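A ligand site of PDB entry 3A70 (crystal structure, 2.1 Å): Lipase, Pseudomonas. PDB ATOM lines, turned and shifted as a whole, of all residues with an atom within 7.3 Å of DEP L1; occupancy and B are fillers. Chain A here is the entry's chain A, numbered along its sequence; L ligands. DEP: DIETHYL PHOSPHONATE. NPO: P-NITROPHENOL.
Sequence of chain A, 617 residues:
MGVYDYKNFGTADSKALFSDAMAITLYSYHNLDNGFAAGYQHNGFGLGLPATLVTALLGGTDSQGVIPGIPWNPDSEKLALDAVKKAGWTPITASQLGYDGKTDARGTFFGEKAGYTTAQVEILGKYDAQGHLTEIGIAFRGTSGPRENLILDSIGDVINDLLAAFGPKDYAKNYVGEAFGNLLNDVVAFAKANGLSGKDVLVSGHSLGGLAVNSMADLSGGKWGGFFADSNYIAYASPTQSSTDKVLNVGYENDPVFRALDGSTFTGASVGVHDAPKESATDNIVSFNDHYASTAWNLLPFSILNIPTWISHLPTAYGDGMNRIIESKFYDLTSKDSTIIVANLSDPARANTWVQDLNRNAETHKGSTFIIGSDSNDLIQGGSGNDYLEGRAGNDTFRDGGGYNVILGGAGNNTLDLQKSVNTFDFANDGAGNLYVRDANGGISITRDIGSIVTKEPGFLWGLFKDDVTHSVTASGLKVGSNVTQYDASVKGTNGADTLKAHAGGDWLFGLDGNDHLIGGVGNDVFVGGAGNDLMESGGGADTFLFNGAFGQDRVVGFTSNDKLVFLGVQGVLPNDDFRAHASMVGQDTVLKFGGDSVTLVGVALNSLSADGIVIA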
ATOM      1  N   TYR A  29       8.031   2.677  -8.621  1.00  0.00           N
ATOM      2  CA  TYR A  29       8.418   1.393  -8.050  1.00  0.00           C
ATOM      3  C   TYR A  29       9.957   1.149  -8.107  1.00  0.00           C
ATOM      4  O   TYR A  29      10.454   0.237  -7.515  1.00  0.00           O
ATOM      5  CB  TYR A  29       7.697   0.259  -8.770  1.00  0.00           C
ATOM      6  CG  TYR A  29       6.247  -0.029  -8.350  1.00  0.00           C
ATOM      7  CD1 TYR A  29       5.949  -0.495  -7.059  1.00  0.00           C
ATOM      8  CD2 TYR A  29       5.200   0.059  -9.268  1.00  0.00           C
ATOM      9  CE1 TYR A  29       4.649  -0.802  -6.688  1.00  0.00           C
ATOM     10  CE2 TYR A  29       3.894  -0.264  -8.899  1.00  0.00           C
ATOM     11  CZ  TYR A  29       3.640  -0.708  -7.620  1.00  0.00           C
ATOM     12  OH  TYR A  29       2.384  -1.052  -7.235  1.00  0.00           O
ATOM     13  N   ARG A 141       3.183   5.629  -5.223  1.00  0.00           N
ATOM     14  CA  ARG A 141       3.682   4.252  -5.180  1.00  0.00           C
ATOM     15  C   ARG A 141       2.637   3.249  -4.667  1.00  0.00           C
ATOM     16  O   ARG A 141       1.893   3.515  -3.708  1.00  0.00           O
ATOM     17  CB  ARG A 141       4.952   4.175  -4.324  1.00  0.00           C
ATOM     18  CG  ARG A 141       5.709   2.858  -4.524  1.00  0.00           C
ATOM     19  CD  ARG A 141       6.932   2.670  -3.588  1.00  0.00           C
ATOM     20  NE  ARG A 141       7.449   1.344  -3.875  1.00  0.00           N
ATOM     21  CZ  ARG A 141       8.704   1.057  -4.188  1.00  0.00           C
ATOM     22  NH1 ARG A 141       9.648   1.978  -4.161  1.00  0.00           N
ATOM     23  NH2 ARG A 141       9.005  -0.209  -4.495  1.00  0.00           N
ATOM     24  N   GLY A 142       2.558   2.082  -5.320  1.00  0.00           N
ATOM     25  CA  GLY A 142       1.775   0.980  -4.763  1.00  0.00           C
ATOM     26  C   GLY A 142       2.368   0.317  -3.533  1.00  0.00           C
ATOM     27  O   GLY A 142       3.381   0.765  -3.023  1.00  0.00           O
ATOM     28  N   THR A 143       1.725  -0.742  -3.037  1.00  0.00           N
ATOM     29  CA  THR A 143       2.289  -1.508  -1.934  1.00  0.00           C
ATOM     30  C   THR A 143       3.753  -1.824  -2.294  1.00  0.00           C
ATOM     31  O   THR A 143       4.069  -2.134  -3.429  1.00  0.00           O
ATOM     32  CB  THR A 143       1.363  -2.734  -1.522  1.00  0.00           C
ATOM     33  OG1 THR A 143       0.085  -2.248  -1.096  1.00  0.00           O
ATOM     34  CG2 THR A 143       1.965  -3.528  -0.403  1.00  0.00           C
ATOM     35  N   SER A 144       4.630  -1.851  -1.307  1.00  0.00           N
ATOM     36  CA  SER A 144       6.095  -1.856  -1.365  1.00  0.00           C
ATOM     37  C   SER A 144       6.782  -0.500  -0.989  1.00  0.00           C
ATOM     38  O   SER A 144       6.161   0.473  -1.058  1.00  0.00           O
ATOM     39  CB  SER A 144       6.679  -2.421  -2.688  1.00  0.00           C
ATOM     40  OG  SER A 144       6.499  -1.558  -3.743  1.00  0.00           O
ATOM     41  N   ASP A 157       2.051  -0.420   4.431  1.00  0.00           N
ATOM     42  CA  ASP A 157       1.191  -0.394   3.227  1.00  0.00           C
ATOM     43  C   ASP A 157       0.014  -1.382   3.327  1.00  0.00           C
ATOM     44  O   ASP A 157      -1.103  -1.022   3.017  1.00  0.00           O
ATOM     45  CB  ASP A 157       1.997  -0.741   1.974  1.00  0.00           C
ATOM     46  CG  ASP A 157       3.024   0.309   1.615  1.00  0.00           C
ATOM     47  OD1 ASP A 157       3.958  -0.009   0.821  1.00  0.00           O
ATOM     48  OD2 ASP A 157       2.912   1.453   2.101  1.00  0.00           O
ATOM     49  N   VAL A 158       0.270  -2.614   3.743  1.00  0.00           N
ATOM     50  CA  VAL A 158      -0.804  -3.651   3.826  1.00  0.00           C
ATOM     51  C   VAL A 158      -1.890  -3.267   4.819  1.00  0.00           C
ATOM     52  O   VAL A 158      -3.091  -3.497   4.547  1.00  0.00           O
ATOM     53  CB  VAL A 158      -0.259  -5.091   4.105  1.00  0.00           C
ATOM     54  CG1 VAL A 158      -1.402  -6.119   4.351  1.00  0.00           C
ATOM     55  CG2 VAL A 158       0.545  -5.553   2.960  1.00  0.00           C
ATOM     56  N   ASP A 161      -3.919  -0.938   2.994  1.00  0.00           N
ATOM     57  CA  ASP A 161      -4.705  -1.725   2.023  1.00  0.00           C
ATOM     58  C   ASP A 161      -5.928  -2.318   2.715  1.00  0.00           C
ATOM     59  O   ASP A 161      -7.012  -2.251   2.183  1.00  0.00           O
ATOM     60  CB  ASP A 161      -3.897  -2.872   1.363  1.00  0.00           C
ATOM     61  CG  ASP A 161      -2.718  -2.387   0.531  1.00  0.00           C
ATOM     62  OD1 ASP A 161      -2.797  -1.309  -0.107  1.00  0.00           O
ATOM     63  OD2 ASP A 161      -1.720  -3.152   0.461  1.00  0.00           O
ATOM     64  N   LEU A 162      -5.703  -2.920   3.875  1.00  0.00           N
ATOM     65  CA  LEU A 162      -6.808  -3.516   4.626  1.00  0.00           C
ATOM     66  C   LEU A 162      -7.822  -2.445   5.096  1.00  0.00           C
ATOM     67  O   LEU A 162      -9.027  -2.689   5.109  1.00  0.00           O
ATOM     68  CB  LEU A 162      -6.278  -4.326   5.829  1.00  0.00           C
ATOM     69  CG  LEU A 162      -5.522  -5.591   5.442  1.00  0.00           C
ATOM     70  CD1 LEU A 162      -4.804  -6.151   6.662  1.00  0.00           C
ATOM     71  CD2 LEU A 162      -6.470  -6.584   4.775  1.00  0.00           C
ATOM     72  N   HIS A 206      -0.031   2.867  -9.418  1.00  0.00           N
ATOM     73  CA  HIS A 206      -0.452   1.461  -9.666  1.00  0.00           C
ATOM     74  C   HIS A 206      -0.863   0.875  -8.327  1.00  0.00           C
ATOM     75  O   HIS A 206      -0.175   1.092  -7.325  1.00  0.00           O
ATOM     76  CB  HIS A 206       0.751   0.715 -10.257  1.00  0.00           C
ATOM     77  CG  HIS A 206       0.563  -0.750 -10.489  1.00  0.00           C
ATOM     78  ND1 HIS A 206       0.898  -1.705  -9.551  1.00  0.00           N
ATOM     79  CD2 HIS A 206       0.190  -1.431 -11.599  1.00  0.00           C
ATOM     80  CE1 HIS A 206       0.700  -2.903 -10.062  1.00  0.00           C
ATOM     81  NE2 HIS A 206       0.268  -2.773 -11.297  1.00  0.00           N
ATOM     82  N   SER A 207      -1.955   0.102  -8.346  1.00  0.00           N
ATOM     83  CA  SER A 207      -2.370  -0.649  -7.196  1.00  0.00           C
ATOM     84  C   SER A 207      -2.799   0.274  -6.047  1.00  0.00           C
ATOM     85  O   SER A 207      -3.705   1.089  -6.264  1.00  0.00           O
ATOM     86  CB  SER A 207      -1.240  -1.598  -6.801  1.00  0.00           C
ATOM     87  OG  SER A 207      -1.746  -2.569  -5.923  1.00  0.00           O
ATOM     88  N   LEU A 208      -2.168   0.190  -4.878  1.00  0.00           N
ATOM     89  CA  LEU A 208      -2.381   1.183  -3.793  1.00  0.00           C
ATOM     90  C   LEU A 208      -2.124   2.615  -4.310  1.00  0.00           C
ATOM     91  O   LEU A 208      -2.779   3.544  -3.882  1.00  0.00           O
ATOM     92  CB  LEU A 208      -1.489   0.906  -2.568  1.00  0.00           C
ATOM     93  CG  LEU A 208      -1.498   1.932  -1.428  1.00  0.00           C
ATOM     94  CD1 LEU A 208      -2.952   2.175  -0.836  1.00  0.00           C
ATOM     95  CD2 LEU A 208      -0.475   1.522  -0.323  1.00  0.00           C
ATOM     96  N   GLY A 209      -1.144   2.779  -5.195  1.00  0.00           N
ATOM     97  CA  GLY A 209      -0.906   4.067  -5.879  1.00  0.00           C
ATOM     98  C   GLY A 209      -2.053   4.456  -6.809  1.00  0.00           C
ATOM     99  O   GLY A 209      -2.384   5.637  -6.972  1.00  0.00           O
ATOM    100  N   GLY A 210      -2.690   3.455  -7.414  1.00  0.00           N
ATOM    101  CA  GLY A 210      -3.874   3.722  -8.209  1.00  0.00           C
ATOM    102  C   GLY A 210      -5.054   4.061  -7.311  1.00  0.00           C
ATOM    103  O   GLY A 210      -5.882   4.877  -7.704  1.00  0.00           O
ATOM    104  N   LEU A 211      -5.152   3.428  -6.124  1.00  0.00           N
ATOM    105  CA  LEU A 211      -6.106   3.837  -5.086  1.00  0.00           C
ATOM    106  C   LEU A 211      -5.900   5.319  -4.758  1.00  0.00           C
ATOM    107  O   LEU A 211      -6.871   6.061  -4.676  1.00  0.00           O
ATOM    108  CB  LEU A 211      -5.942   3.010  -3.800  1.00  0.00           C
ATOM    109  CG  LEU A 211      -6.839   3.373  -2.591  1.00  0.00           C
ATOM    110  CD1 LEU A 211      -6.914   2.188  -1.696  1.00  0.00           C
ATOM    111  CD2 LEU A 211      -6.287   4.592  -1.799  1.00  0.00           C
ATOM    112  N   ALA A 237      -4.488  -0.620 -12.143  1.00  0.00           N
ATOM    113  CA  ALA A 237      -4.687  -1.712 -11.181  1.00  0.00           C
ATOM    114  C   ALA A 237      -5.189  -1.235  -9.804  1.00  0.00           C
ATOM    115  O   ALA A 237      -4.835  -1.807  -8.766  1.00  0.00           O
ATOM    116  CB  ALA A 237      -3.390  -2.519 -11.009  1.00  0.00           C
ATOM    117  N   SER A 238      -5.970  -0.178  -9.780  1.00  0.00           N
ATOM    118  CA  SER A 238      -6.521   0.311  -8.538  1.00  0.00           C
ATOM    119  C   SER A 238      -7.612  -0.666  -8.078  1.00  0.00           C
ATOM    120  O   SER A 238      -8.420  -1.106  -8.891  1.00  0.00           O
ATOM    121  CB  SER A 238      -7.120   1.723  -8.732  1.00  0.00           C
ATOM    122  OG  SER A 238      -7.807   2.202  -7.584  1.00  0.00           O
ATOM    123  N   PRO A 239      -7.624  -1.011  -6.781  1.00  0.00           N
ATOM    124  CA  PRO A 239      -8.809  -1.703  -6.241  1.00  0.00           C
ATOM    125  C   PRO A 239     -10.073  -0.828  -6.140  1.00  0.00           C
ATOM    126  O   PRO A 239     -11.195  -1.367  -6.022  1.00  0.00           O
ATOM    127  CB  PRO A 239      -8.324  -2.143  -4.847  1.00  0.00           C
ATOM    128  CG  PRO A 239      -7.224  -1.079  -4.481  1.00  0.00           C
ATOM    129  CD  PRO A 239      -6.550  -0.836  -5.767  1.00  0.00           C
ATOM    130  N   VAL A 257      -6.260  -7.675  -8.180  1.00  0.00           N
ATOM    131  CA  VAL A 257      -6.288  -6.376  -7.463  1.00  0.00           C
ATOM    132  C   VAL A 257      -7.227  -5.382  -8.114  1.00  0.00           C
ATOM    133  O   VAL A 257      -7.877  -4.579  -7.426  1.00  0.00           O
ATOM    134  CB  VAL A 257      -4.862  -5.713  -7.334  1.00  0.00           C
ATOM    135  CG1 VAL A 257      -4.955  -4.284  -6.570  1.00  0.00           C
ATOM    136  CG2 VAL A 257      -3.912  -6.644  -6.584  1.00  0.00           C
ATOM    137  N   ALA A 260     -11.114  -4.819  -7.245  1.00  0.00           N
ATOM    138  CA  ALA A 260     -11.425  -5.693  -6.112  1.00  0.00           C
ATOM    139  C   ALA A 260     -12.536  -5.063  -5.298  1.00  0.00           C
ATOM    140  O   ALA A 260     -13.419  -5.747  -4.830  1.00  0.00           O
ATOM    141  CB  ALA A 260     -10.211  -5.921  -5.226  1.00  0.00           C
ATOM    142  N   ILE A 304      -7.879 -12.732  -5.292  1.00  0.00           N
ATOM    143  CA  ILE A 304      -6.832 -11.919  -4.675  1.00  0.00           C
ATOM    144  C   ILE A 304      -6.097 -12.665  -3.505  1.00  0.00           C
ATOM    145  O   ILE A 304      -4.960 -12.303  -3.156  1.00  0.00           O
ATOM    146  CB  ILE A 304      -7.421 -10.508  -4.267  1.00  0.00           C
ATOM    147  CG1 ILE A 304      -6.292  -9.461  -4.124  1.00  0.00           C
ATOM    148  CG2 ILE A 304      -8.434 -10.595  -3.087  1.00  0.00           C
ATOM    149  CD1 ILE A 304      -6.784  -8.014  -3.881  1.00  0.00           C
ATOM    150  N   TRP A 310      -1.419 -13.136  -8.740  1.00  0.00           N
ATOM    151  CA  TRP A 310      -0.845 -11.769  -8.766  1.00  0.00           C
ATOM    152  C   TRP A 310       0.213 -11.590  -9.832  1.00  0.00           C
ATOM    153  O   TRP A 310       0.702 -10.469 -10.049  1.00  0.00           O
ATOM    154  CB  TRP A 310      -0.212 -11.402  -7.398  1.00  0.00           C
ATOM    155  CG  TRP A 310      -1.222 -11.081  -6.294  1.00  0.00           C
ATOM    156  CD1 TRP A 310      -2.178 -11.916  -5.793  1.00  0.00           C
ATOM    157  CD2 TRP A 310      -1.333  -9.848  -5.553  1.00  0.00           C
ATOM    158  NE1 TRP A 310      -2.892 -11.274  -4.804  1.00  0.00           N
ATOM    159  CE2 TRP A 310      -2.402 -10.007  -4.636  1.00  0.00           C
ATOM    160  CE3 TRP A 310      -0.628  -8.628  -5.585  1.00  0.00           C
ATOM    161  CZ2 TRP A 310      -2.781  -8.997  -3.714  1.00  0.00           C
ATOM    162  CZ3 TRP A 310      -1.026  -7.593  -4.698  1.00  0.00           C
ATOM    163  CH2 TRP A 310      -2.106  -7.799  -3.781  1.00  0.00           C
ATOM    164  N   HIS A 313      -0.636  -8.883 -12.033  1.00  0.00           N
ATOM    165  CA  HIS A 313      -0.554  -7.597 -11.385  1.00  0.00           C
ATOM    166  C   HIS A 313       0.784  -6.870 -11.616  1.00  0.00           C
ATOM    167  O   HIS A 313       0.821  -5.664 -11.484  1.00  0.00           O
ATOM    168  CB  HIS A 313      -0.809  -7.781  -9.873  1.00  0.00           C
ATOM    169  CG  HIS A 313      -0.893  -6.499  -9.106  1.00  0.00           C
ATOM    170  ND1 HIS A 313      -1.846  -5.532  -9.347  1.00  0.00           N
ATOM    171  CD2 HIS A 313      -0.137  -6.021  -8.069  1.00  0.00           C
ATOM    172  CE1 HIS A 313      -1.680  -4.525  -8.495  1.00  0.00           C
ATOM    173  NE2 HIS A 313      -0.646  -4.801  -7.717  1.00  0.00           N
ATOM    174  N   PRO A 315       3.896  -4.708 -12.298  1.00  0.00           N
ATOM    175  CA  PRO A 315       3.926  -3.459 -13.031  1.00  0.00           C
ATOM    176  C   PRO A 315       4.717  -3.546 -14.373  1.00  0.00           C
ATOM    177  O   PRO A 315       4.295  -2.921 -15.299  1.00  0.00           O
ATOM    178  CB  PRO A 315       4.516  -2.466 -12.021  1.00  0.00           C
ATOM    179  CG  PRO A 315       5.105  -3.246 -10.970  1.00  0.00           C
ATOM    180  CD  PRO A 315       4.498  -4.606 -10.958  1.00  0.00           C
HETATM  181  C1  DEP L   1       1.309  -3.789  -5.321  1.00  0.00           C
HETATM  182  C2  DEP L   1       2.194  -5.025  -5.064  1.00  0.00           C
HETATM  183  C3  DEP L   1      -3.534  -3.359  -3.315  1.00  0.00           C
HETATM  184  C4  DEP L   1      -4.292  -4.275  -2.369  1.00  0.00           C
HETATM  185  O1  DEP L   1       0.062  -4.117  -4.677  1.00  0.00           O
HETATM  186  O2  DEP L   1      -2.261  -3.938  -3.591  1.00  0.00           O
HETATM  187  O3  DEP L   1      -0.601  -1.870  -3.730  1.00  0.00           O
HETATM  188  P   DEP L   1      -1.181  -3.132  -4.490  1.00  0.00           P
HETATM  189  C1  NPO L   2       6.653  -6.466  -6.416  1.00  0.00           C
HETATM  190  C2  NPO L   2       6.229  -7.640  -5.774  1.00  0.00           C
HETATM  191  C3  NPO L   2       7.111  -8.692  -5.574  1.00  0.00           C
HETATM  192  C4  NPO L   2       8.435  -8.592  -5.994  1.00  0.00           C
HETATM  193  C5  NPO L   2       8.867  -7.429  -6.625  1.00  0.00           C
HETATM  194  C6  NPO L   2       7.984  -6.377  -6.825  1.00  0.00           C
HETATM  195  OH  NPO L   2       9.311  -9.624  -5.796  1.00  0.00           O
HETATM  196  N1  NPO L   2       5.755  -5.405  -6.633  1.00  0.00           N
HETATM  197  O2  NPO L   2       6.105  -4.308  -7.056  1.00  0.00           O
HETATM  198  O3  NPO L   2       4.566  -5.596  -6.413  1.00  0.00           O
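A ring nitrogen (NE2) of His 206 sits at hydrogen-bond distance from the backbone carbonyl oxygen (O) of His 313. O of Ile 304 sits at hydrogen-bond distance from NE1 of Trp 310, 2.8 Å away. The backbone carbonyl oxygen (O) of Ala 237 sits close to the backbone NH (N) of Ser 207, 3.5 Å away. The backbone carbonyl oxygen (O) of Tyr 29 is in hydrogen-bond range of the guanidinium group (NH2) of Arg 141. The side-chain hydroxyl (OG1) of Thr 143 lies within hydrogen-bond range of the side-chain carboxylate (OD2) of Asp 161 (2.5 Å). The side-chain hydroxyl (OG) of Ser 207 is in hydrogen-bond range of a ring nitrogen (NE2) of His 313 (3.1 Å). A ring nitrogen (ND1) of His 206 lies within hydrogen-bond range of the side-chain hydroxyl of Tyr 29, at 2.8 Å.
Tyr 29 touches DEP L1. Gly 142 touches DEP L1. Asp 161 touches DEP L1 (CG to C4, 3.8 Å). Val 257 touches DEP L1 (CG1 to C3, 3.7 Å). Trp 310 touches DEP L1. Hydrophobic or aromatic side chains within 4 Å of DEP L1: Leu 208, Val 257, Trp 310 and His 313. Within 4 Å of DEP L1: Tyr 29, Gly 142, Thr 143, Asp 161, Ser 207, Leu 208, Val 257, Trp 310 and His 313.
The backbone NH of Leu 208 is in hydrogen-bond range of an oxygen (O3) of DEP L1. An oxygen (O3) of DEP L1 lies within hydrogen-bond range of the side-chain hydroxyl of Thr 143 (2.7 Å). A phosphorus (P) of DEP L1 is bonded to the side-chain hydroxyl (OG) of Ser 207 (1.6 Å). O3 of DEP L1 lies within hydrogen-bond range of N of Thr 143, 2.7 Å away. A ring nitrogen (NE2) of His 313 sits at hydrogen-bond distance from an oxygen (O1) of DEP L1 (3.2 Å).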
